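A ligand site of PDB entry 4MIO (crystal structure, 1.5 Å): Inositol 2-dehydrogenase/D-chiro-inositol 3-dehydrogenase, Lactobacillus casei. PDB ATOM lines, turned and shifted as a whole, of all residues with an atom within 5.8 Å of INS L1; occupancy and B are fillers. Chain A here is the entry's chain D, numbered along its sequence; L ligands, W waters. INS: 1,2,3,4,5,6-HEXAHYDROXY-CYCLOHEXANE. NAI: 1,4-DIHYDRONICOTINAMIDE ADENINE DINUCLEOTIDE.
O7N of NAI L2 is in hydrogen-bond range of O3 of INS L1, at 2.8 Å.
The side-chain amino group of Lys 97 lies within hydrogen-bond range of an oxygen (O2) of INS L1, 2.6 Å away.
O4 of INS L1 lies within hydrogen-bond range of NE2 of His 155, 2.7 Å away.
An oxygen (O7N) of NAI L2 is in hydrogen-bond range of the side-chain hydroxyl (OH) of Tyr 282, at 2.4 Å.
O5 of INS L1 is in hydrogen-bond range of OD1 of Asn 157 (2.6 Å).
O4 of INS L1 lies within hydrogen-bond range of OH of Tyr 236 (2.7 Å).
An oxygen (O2) of INS L1 is in hydrogen-bond range of the backbone carbonyl oxygen (O) of Asp 172, at 3.0 Å.
The side-chain carboxylate (OD1) of Asp 172 lies within hydrogen-bond range of an oxygen (O2D) of NAI L2 (2.9 Å).
The side-chain sulfur (SD) of Met 126 is in hydrogen-bond range of a nitrogen (N7N) of NAI L2.
The backbone carbonyl oxygen (O) of Lys 97 lies within hydrogen-bond range of an oxygen (O3D) of NAI L2, 2.9 Å away.
O2 of INS L1 lies within hydrogen-bond range of NE2 of His 176 (2.9 Å).
O6 of INS L1 sits at hydrogen-bond distance from OD2 of Asp 172 (3.0 Å).
The side-chain hydroxyl (OG1) of Thr 173 lies within hydrogen-bond range of an oxygen (O5) of INS L1.
An oxygen (O2D) of NAI L2 lies within hydrogen-bond range of the side-chain amino group (NZ) of Lys 97 (2.8 Å).
Water W2 lies within hydrogen-bond range of an oxygen (O1) of INS L1 and an oxygen (O1N) of NAI L2.
Water W3 lies within hydrogen-bond range of OH of Tyr 236, O3 of INS L1 and NH2 of Arg 127.
Residues that only touch INS L1: Tyr 164 (3.95 Å).
Of the 15 residues printed, 8 come within 4 Å of INS L1.
The nearest printed residue that does not touch INS L1 is Met 126 (4.1 Å).
The side-chain amino group (NZ) of Lys 97 is in salt-bridge range of the side-chain carboxylate (OD1) of Asp 172 (3.6 Å).
The side-chain hydroxyl (OG1) of Thr 173 sits at hydrogen-bond distance from the side-chain hydroxyl (OH) of Tyr 164, at 2.6 Å.
ND1 of His 155 lies close to NH2 of Arg 127, at 3.4 Å.
A ring nitrogen (ND1) of His 155 sits close to the backbone carbonyl oxygen (O) of Thr 173, at 3.2 Å.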
ATOM      1  N   LYS A  97      -2.512   6.572  -5.282  1.00  0.00           N
ATOM      2  CA  LYS A  97      -1.426   5.845  -5.868  1.00  0.00           C
ATOM      3  C   LYS A  97      -0.778   6.610  -7.054  1.00  0.00           C
ATOM      4  O   LYS A  97      -1.370   7.459  -7.617  1.00  0.00           O
ATOM      5  CB  LYS A  97      -1.853   4.432  -6.253  1.00  0.00           C
ATOM      6  CG  LYS A  97      -3.166   4.269  -6.939  1.00  0.00           C
ATOM      7  CD  LYS A  97      -3.349   5.047  -8.159  1.00  0.00           C
ATOM      8  CE  LYS A  97      -2.406   4.709  -9.262  1.00  0.00           C
ATOM      9  NZ  LYS A  97      -2.801   5.462 -10.486  1.00  0.00           N
ATOM     10  N   MET A 126      -7.645   1.400  -4.186  1.00  0.00           N
ATOM     11  CA  MET A 126      -9.065   1.209  -3.987  1.00  0.00           C
ATOM     12  C   MET A 126      -9.586  -0.172  -4.383  1.00  0.00           C
ATOM     13  O   MET A 126     -10.660  -0.507  -4.019  1.00  0.00           O
ATOM     14  CB  MET A 126      -9.883   2.289  -4.717  1.00  0.00           C
ATOM     15  CG  MET A 126     -10.191   2.027  -6.157  1.00  0.00           C
ATOM     16  SD  MET A 126      -8.693   2.041  -7.126  1.00  0.00           S
ATOM     17  CE  MET A 126      -9.350   1.740  -8.772  1.00  0.00           C
ATOM     18  N   ARG A 127      -8.817  -0.895  -5.173  1.00  0.00           N
ATOM     19  CA  ARG A 127      -9.289  -2.186  -5.654  1.00  0.00           C
ATOM     20  C   ARG A 127      -9.753  -3.123  -4.523  1.00  0.00           C
ATOM     21  O   ARG A 127     -10.698  -3.822  -4.672  1.00  0.00           O
ATOM     22  CB  ARG A 127      -8.255  -2.916  -6.520  1.00  0.00           C
ATOM     23  CG  ARG A 127      -7.830  -2.241  -7.837  1.00  0.00           C
ATOM     24  CD  ARG A 127      -8.850  -2.368  -8.954  1.00  0.00           C
ATOM     25  NE  ARG A 127      -8.362  -1.848 -10.176  1.00  0.00           N
ATOM     26  CZ  ARG A 127      -7.615  -2.500 -11.025  1.00  0.00           C
ATOM     27  NH1 ARG A 127      -7.301  -3.748 -10.788  1.00  0.00           N
ATOM     28  NH2 ARG A 127      -7.195  -1.923 -12.114  1.00  0.00           N
ATOM     29  N   HIS A 155      -6.394  -4.727 -17.592  1.00  0.00           N
ATOM     30  CA  HIS A 155      -6.529  -3.342 -17.187  1.00  0.00           C
ATOM     31  C   HIS A 155      -6.577  -2.496 -18.478  1.00  0.00           C
ATOM     32  O   HIS A 155      -5.617  -2.292 -19.110  1.00  0.00           O
ATOM     33  CB  HIS A 155      -5.359  -2.946 -16.325  1.00  0.00           C
ATOM     34  CG  HIS A 155      -5.536  -1.679 -15.589  1.00  0.00           C
ATOM     35  ND1 HIS A 155      -4.817  -1.364 -14.479  1.00  0.00           N
ATOM     36  CD2 HIS A 155      -6.355  -0.640 -15.804  1.00  0.00           C
ATOM     37  CE1 HIS A 155      -5.188  -0.188 -14.036  1.00  0.00           C
ATOM     38  NE2 HIS A 155      -6.118   0.281 -14.826  1.00  0.00           N
ATOM     39  N   ILE A 156      -7.804  -2.122 -18.810  1.00  0.00           N
ATOM     40  CA  ILE A 156      -8.091  -1.502 -20.077  1.00  0.00           C
ATOM     41  C   ILE A 156      -8.507  -0.034 -19.885  1.00  0.00           C
ATOM     42  O   ILE A 156      -9.330   0.243 -19.096  1.00  0.00           O
ATOM     43  CB  ILE A 156      -9.272  -2.210 -20.756  1.00  0.00           C
ATOM     44  CG1 ILE A 156      -9.045  -3.710 -20.885  1.00  0.00           C
ATOM     45  CG2 ILE A 156      -9.540  -1.580 -22.087  1.00  0.00           C
ATOM     46  CD1 ILE A 156      -7.827  -4.126 -21.648  1.00  0.00           C
ATOM     47  N   ASN A 157      -7.893   0.859 -20.657  1.00  0.00           N
ATOM     48  CA  ASN A 157      -8.289   2.258 -20.692  1.00  0.00           C
ATOM     49  C   ASN A 157      -8.506   2.615 -22.165  1.00  0.00           C
ATOM     50  O   ASN A 157      -7.904   2.059 -23.001  1.00  0.00           O
ATOM     51  CB  ASN A 157      -7.204   3.204 -20.201  1.00  0.00           C
ATOM     52  CG  ASN A 157      -6.793   3.035 -18.771  1.00  0.00           C
ATOM     53  OD1 ASN A 157      -5.840   3.631 -18.377  1.00  0.00           O
ATOM     54  ND2 ASN A 157      -7.494   2.256 -18.013  1.00  0.00           N
ATOM     55  N   TYR A 164       1.292  10.962 -20.305  1.00  0.00           N
ATOM     56  CA  TYR A 164       1.398   9.566 -19.909  1.00  0.00           C
ATOM     57  C   TYR A 164       2.613   8.901 -20.563  1.00  0.00           C
ATOM     58  O   TYR A 164       2.711   8.855 -21.747  1.00  0.00           O
ATOM     59  CB  TYR A 164       0.111   8.827 -20.250  1.00  0.00           C
ATOM     60  CG  TYR A 164      -0.061   7.416 -19.694  1.00  0.00           C
ATOM     61  CD1 TYR A 164       0.550   6.344 -20.287  1.00  0.00           C
ATOM     62  CD2 TYR A 164      -0.846   7.177 -18.598  1.00  0.00           C
ATOM     63  CE1 TYR A 164       0.408   5.102 -19.822  1.00  0.00           C
ATOM     64  CE2 TYR A 164      -1.001   5.909 -18.119  1.00  0.00           C
ATOM     65  CZ  TYR A 164      -0.391   4.868 -18.743  1.00  0.00           C
ATOM     66  OH  TYR A 164      -0.560   3.612 -18.273  1.00  0.00           O
ATOM     67  N   ASP A 172       1.337   4.061 -12.797  1.00  0.00           N
ATOM     68  CA  ASP A 172      -0.004   4.622 -12.764  1.00  0.00           C
ATOM     69  C   ASP A 172      -1.073   3.550 -13.006  1.00  0.00           C
ATOM     70  O   ASP A 172      -2.144   3.657 -12.539  1.00  0.00           O
ATOM     71  CB  ASP A 172      -0.122   5.718 -13.842  1.00  0.00           C
ATOM     72  CG  ASP A 172      -0.754   6.990 -13.355  1.00  0.00           C
ATOM     73  OD1 ASP A 172      -0.428   7.451 -12.288  1.00  0.00           O
ATOM     74  OD2 ASP A 172      -1.628   7.491 -14.085  1.00  0.00           O
ATOM     75  N   THR A 173      -0.709   2.515 -13.741  1.00  0.00           N
ATOM     76  CA  THR A 173      -1.687   1.578 -14.235  1.00  0.00           C
ATOM     77  C   THR A 173      -1.512   0.150 -13.629  1.00  0.00           C
ATOM     78  O   THR A 173      -2.279  -0.236 -12.830  1.00  0.00           O
ATOM     79  CB  THR A 173      -1.737   1.572 -15.786  1.00  0.00           C
ATOM     80  OG1 THR A 173      -2.045   2.882 -16.230  1.00  0.00           O
ATOM     81  CG2 THR A 173      -2.771   0.649 -16.309  1.00  0.00           C
ATOM     82  N   HIS A 176      -2.013  -1.005  -9.792  1.00  0.00           N
ATOM     83  CA  HIS A 176      -3.230  -1.504  -9.190  1.00  0.00           C
ATOM     84  C   HIS A 176      -3.221  -3.040  -9.077  1.00  0.00           C
ATOM     85  O   HIS A 176      -3.574  -3.573  -8.066  1.00  0.00           O
ATOM     86  CB  HIS A 176      -4.457  -1.073  -9.975  1.00  0.00           C
ATOM     87  CG  HIS A 176      -4.848   0.349  -9.763  1.00  0.00           C
ATOM     88  ND1 HIS A 176      -5.380   0.797  -8.586  1.00  0.00           N
ATOM     89  CD2 HIS A 176      -4.741   1.424 -10.556  1.00  0.00           C
ATOM     90  CE1 HIS A 176      -5.611   2.087  -8.683  1.00  0.00           C
ATOM     91  NE2 HIS A 176      -5.225   2.490  -9.858  1.00  0.00           N
ATOM     92  N   VAL A 230      -3.893   0.598 -22.696  1.00  0.00           N
ATOM     93  CA  VAL A 230      -4.341   1.927 -22.325  1.00  0.00           C
ATOM     94  C   VAL A 230      -4.778   2.848 -23.482  1.00  0.00           C
ATOM     95  O   VAL A 230      -5.229   3.926 -23.228  1.00  0.00           O
ATOM     96  CB  VAL A 230      -3.339   2.643 -21.415  1.00  0.00           C
ATOM     97  CG1 VAL A 230      -3.068   1.793 -20.220  1.00  0.00           C
ATOM     98  CG2 VAL A 230      -2.044   2.933 -22.124  1.00  0.00           C
ATOM     99  N   TYR A 236     -13.316   1.607 -20.754  1.00  0.00           N
ATOM    100  CA  TYR A 236     -12.545   1.406 -19.561  1.00  0.00           C
ATOM    101  C   TYR A 236     -13.029   0.124 -18.906  1.00  0.00           C
ATOM    102  O   TYR A 236     -14.183  -0.020 -18.698  1.00  0.00           O
ATOM    103  CB  TYR A 236     -12.735   2.573 -18.586  1.00  0.00           C
ATOM    104  CG  TYR A 236     -11.943   2.446 -17.318  1.00  0.00           C
ATOM    105  CD1 TYR A 236     -12.437   1.747 -16.234  1.00  0.00           C
ATOM    106  CD2 TYR A 236     -10.680   2.979 -17.208  1.00  0.00           C
ATOM    107  CE1 TYR A 236     -11.694   1.592 -15.098  1.00  0.00           C
ATOM    108  CE2 TYR A 236      -9.955   2.852 -16.056  1.00  0.00           C
ATOM    109  CZ  TYR A 236     -10.461   2.159 -15.013  1.00  0.00           C
ATOM    110  OH  TYR A 236      -9.724   2.029 -13.906  1.00  0.00           O
ATOM    111  N   TRP A 274     -12.593   5.384 -15.013  1.00  0.00           N
ATOM    112  CA  TRP A 274     -12.515   4.926 -13.640  1.00  0.00           C
ATOM    113  C   TRP A 274     -13.495   5.653 -12.729  1.00  0.00           C
ATOM    114  O   TRP A 274     -13.905   5.127 -11.731  1.00  0.00           O
ATOM    115  CB  TRP A 274     -11.079   5.165 -13.129  1.00  0.00           C
ATOM    116  CG  TRP A 274     -10.520   6.472 -13.538  1.00  0.00           C
ATOM    117  CD1 TRP A 274      -9.821   6.732 -14.649  1.00  0.00           C
ATOM    118  CD2 TRP A 274     -10.669   7.726 -12.862  1.00  0.00           C
ATOM    119  NE1 TRP A 274      -9.529   8.051 -14.724  1.00  0.00           N
ATOM    120  CE2 TRP A 274     -10.054   8.689 -13.642  1.00  0.00           C
ATOM    121  CE3 TRP A 274     -11.280   8.115 -11.696  1.00  0.00           C
ATOM    122  CZ2 TRP A 274      -9.997  10.024 -13.273  1.00  0.00           C
ATOM    123  CZ3 TRP A 274     -11.257   9.447 -11.341  1.00  0.00           C
ATOM    124  CH2 TRP A 274     -10.617  10.371 -12.117  1.00  0.00           C
ATOM    125  N   PHE A 278     -15.336   2.803 -10.485  1.00  0.00           N
ATOM    126  CA  PHE A 278     -14.860   2.532  -9.124  1.00  0.00           C
ATOM    127  C   PHE A 278     -15.384   3.514  -8.057  1.00  0.00           C
ATOM    128  O   PHE A 278     -14.840   3.613  -7.015  1.00  0.00           O
ATOM    129  CB  PHE A 278     -13.330   2.444  -9.095  1.00  0.00           C
ATOM    130  CG  PHE A 278     -12.810   1.178  -9.686  1.00  0.00           C
ATOM    131  CD1 PHE A 278     -13.035  -0.009  -9.065  1.00  0.00           C
ATOM    132  CD2 PHE A 278     -12.096   1.177 -10.867  1.00  0.00           C
ATOM    133  CE1 PHE A 278     -12.573  -1.167  -9.589  1.00  0.00           C
ATOM    134  CE2 PHE A 278     -11.640   0.000 -11.381  1.00  0.00           C
ATOM    135  CZ  PHE A 278     -11.890  -1.167 -10.740  1.00  0.00           C
ATOM    136  N   TYR A 282     -13.917   4.058  -4.206  1.00  0.00           N
ATOM    137  CA  TYR A 282     -13.392   5.350  -3.765  1.00  0.00           C
ATOM    138  C   TYR A 282     -14.183   5.895  -2.569  1.00  0.00           C
ATOM    139  O   TYR A 282     -13.616   6.356  -1.645  1.00  0.00           O
ATOM    140  CB  TYR A 282     -13.440   6.375  -4.908  1.00  0.00           C
ATOM    141  CG  TYR A 282     -12.701   6.026  -6.188  1.00  0.00           C
ATOM    142  CD1 TYR A 282     -11.440   5.513  -6.168  1.00  0.00           C
ATOM    143  CD2 TYR A 282     -13.293   6.232  -7.394  1.00  0.00           C
ATOM    144  CE1 TYR A 282     -10.793   5.197  -7.328  1.00  0.00           C
ATOM    145  CE2 TYR A 282     -12.646   5.928  -8.561  1.00  0.00           C
ATOM    146  CZ  TYR A 282     -11.412   5.395  -8.545  1.00  0.00           C
ATOM    147  OH  TYR A 282     -10.774   5.102  -9.708  1.00  0.00           O
HETATM  148  C1  INS L   1      -5.376   6.230 -13.527  1.00  0.00           C
HETATM  149  C2  INS L   1      -5.893   5.261 -12.419  1.00  0.00           C
HETATM  150  C3  INS L   1      -6.877   4.329 -13.011  1.00  0.00           C
HETATM  151  C4  INS L   1      -6.138   3.506 -14.076  1.00  0.00           C
HETATM  152  C5  INS L   1      -5.602   4.413 -15.178  1.00  0.00           C
HETATM  153  C6  INS L   1      -4.557   5.400 -14.528  1.00  0.00           C
HETATM  154  O1  INS L   1      -4.479   7.066 -12.911  1.00  0.00           O
HETATM  155  O2  INS L   1      -4.873   4.649 -11.765  1.00  0.00           O
HETATM  156  O3  INS L   1      -7.539   3.510 -11.936  1.00  0.00           O
HETATM  157  O4  INS L   1      -7.201   2.758 -14.677  1.00  0.00           O
HETATM  158  O5  INS L   1      -4.865   3.602 -16.000  1.00  0.00           O
HETATM  159  O6  INS L   1      -3.954   6.320 -15.521  1.00  0.00           O
HETATM  160  PA  NAI L   2      -4.963  15.249 -13.714  1.00  0.00           P
HETATM  161  O1A NAI L   2      -3.912  15.408 -14.685  1.00  0.00           O
HETATM  162  O2A NAI L   2      -6.305  15.422 -14.174  1.00  0.00           O
HETATM  163  O5B NAI L   2      -4.711  16.163 -12.431  1.00  0.00           O
HETATM  164  C5B NAI L   2      -3.467  16.231 -11.839  1.00  0.00           C
HETATM  165  C4B NAI L   2      -3.446  17.582 -11.164  1.00  0.00           C
HETATM  166  O4B NAI L   2      -2.289  17.714 -10.375  1.00  0.00           O
HETATM  167  C3B NAI L   2      -3.371  18.738 -12.145  1.00  0.00           C
HETATM  168  O3B NAI L   2      -4.332  19.709 -11.826  1.00  0.00           O
HETATM  169  C2B NAI L   2      -1.976  19.252 -11.979  1.00  0.00           C
HETATM  170  O2B NAI L   2      -1.842  20.609 -12.315  1.00  0.00           O
HETATM  171  C1B NAI L   2      -1.725  19.003 -10.522  1.00  0.00           C
HETATM  172  N9A NAI L   2      -0.334  18.946 -10.092  1.00  0.00           N
HETATM  173  C8A NAI L   2       0.701  18.425 -10.708  1.00  0.00           C
HETATM  174  N7A NAI L   2       1.787  18.506  -9.957  1.00  0.00           N
HETATM  175  C5A NAI L   2       1.441  19.100  -8.834  1.00  0.00           C
HETATM  176  C6A NAI L   2       2.103  19.445  -7.596  1.00  0.00           C
HETATM  177  N6A NAI L   2       3.410  19.273  -7.464  1.00  0.00           N
HETATM  178  N1A NAI L   2       1.332  19.994  -6.697  1.00  0.00           N
HETATM  179  C2A NAI L   2       0.069  20.213  -6.889  1.00  0.00           C
HETATM  180  N3A NAI L   2      -0.613  19.911  -7.954  1.00  0.00           N
HETATM  181  C4A NAI L   2       0.037  19.349  -8.922  1.00  0.00           C
HETATM  182  O3  NAI L   2      -4.708  13.784 -13.169  1.00  0.00           O
HETATM  183  PN  NAI L   2      -5.654  12.866 -12.251  1.00  0.00           P
HETATM  184  O1N NAI L   2      -6.331  11.905 -13.126  1.00  0.00           O
HETATM  185  O2N NAI L   2      -6.450  13.634 -11.363  1.00  0.00           O
HETATM  186  O5D NAI L   2      -4.628  12.072 -11.422  1.00  0.00           O
HETATM  187  C5D NAI L   2      -4.145  12.547 -10.209  1.00  0.00           C
HETATM  188  C4D NAI L   2      -3.632  11.425  -9.307  1.00  0.00           C
HETATM  189  O4D NAI L   2      -4.707  10.555  -9.046  1.00  0.00           O
HETATM  190  C3D NAI L   2      -2.584  10.486  -9.907  1.00  0.00           C
HETATM  191  O3D NAI L   2      -1.724   9.972  -8.921  1.00  0.00           O
HETATM  192  C2D NAI L   2      -3.398   9.365 -10.462  1.00  0.00           C
HETATM  193  O2D NAI L   2      -2.605   8.205 -10.556  1.00  0.00           O
HETATM  194  C1D NAI L   2      -4.447   9.225  -9.383  1.00  0.00           C
HETATM  195  N1N NAI L   2      -5.645   8.544  -9.820  1.00  0.00           N
HETATM  196  C2N NAI L   2      -6.068   7.445  -9.224  1.00  0.00           C
HETATM  197  C3N NAI L   2      -7.184   6.782  -9.636  1.00  0.00           C
HETATM  198  C7N NAI L   2      -7.630   5.544  -8.967  1.00  0.00           C
HETATM  199  O7N NAI L   2      -8.363   4.838  -9.558  1.00  0.00           O
HETATM  200  N7N NAI L   2      -7.158   5.345  -7.784  1.00  0.00           N
HETATM  201  C4N NAI L   2      -7.990   7.268 -10.788  1.00  0.00           C
HETATM  202  C5N NAI L   2      -7.467   8.480 -11.345  1.00  0.00           C
HETATM  203  C6N NAI L   2      -6.323   9.053 -10.836  1.00  0.00           C
HETATM  204  O   HOH W   1      -4.922   7.831 -17.426  1.00  0.00           O
HETATM  205  O   HOH W   2      -4.836   9.574 -14.105  1.00  0.00           O
HETATM  206  O   HOH W   3      -8.343   0.736 -11.887  1.00  0.00           O
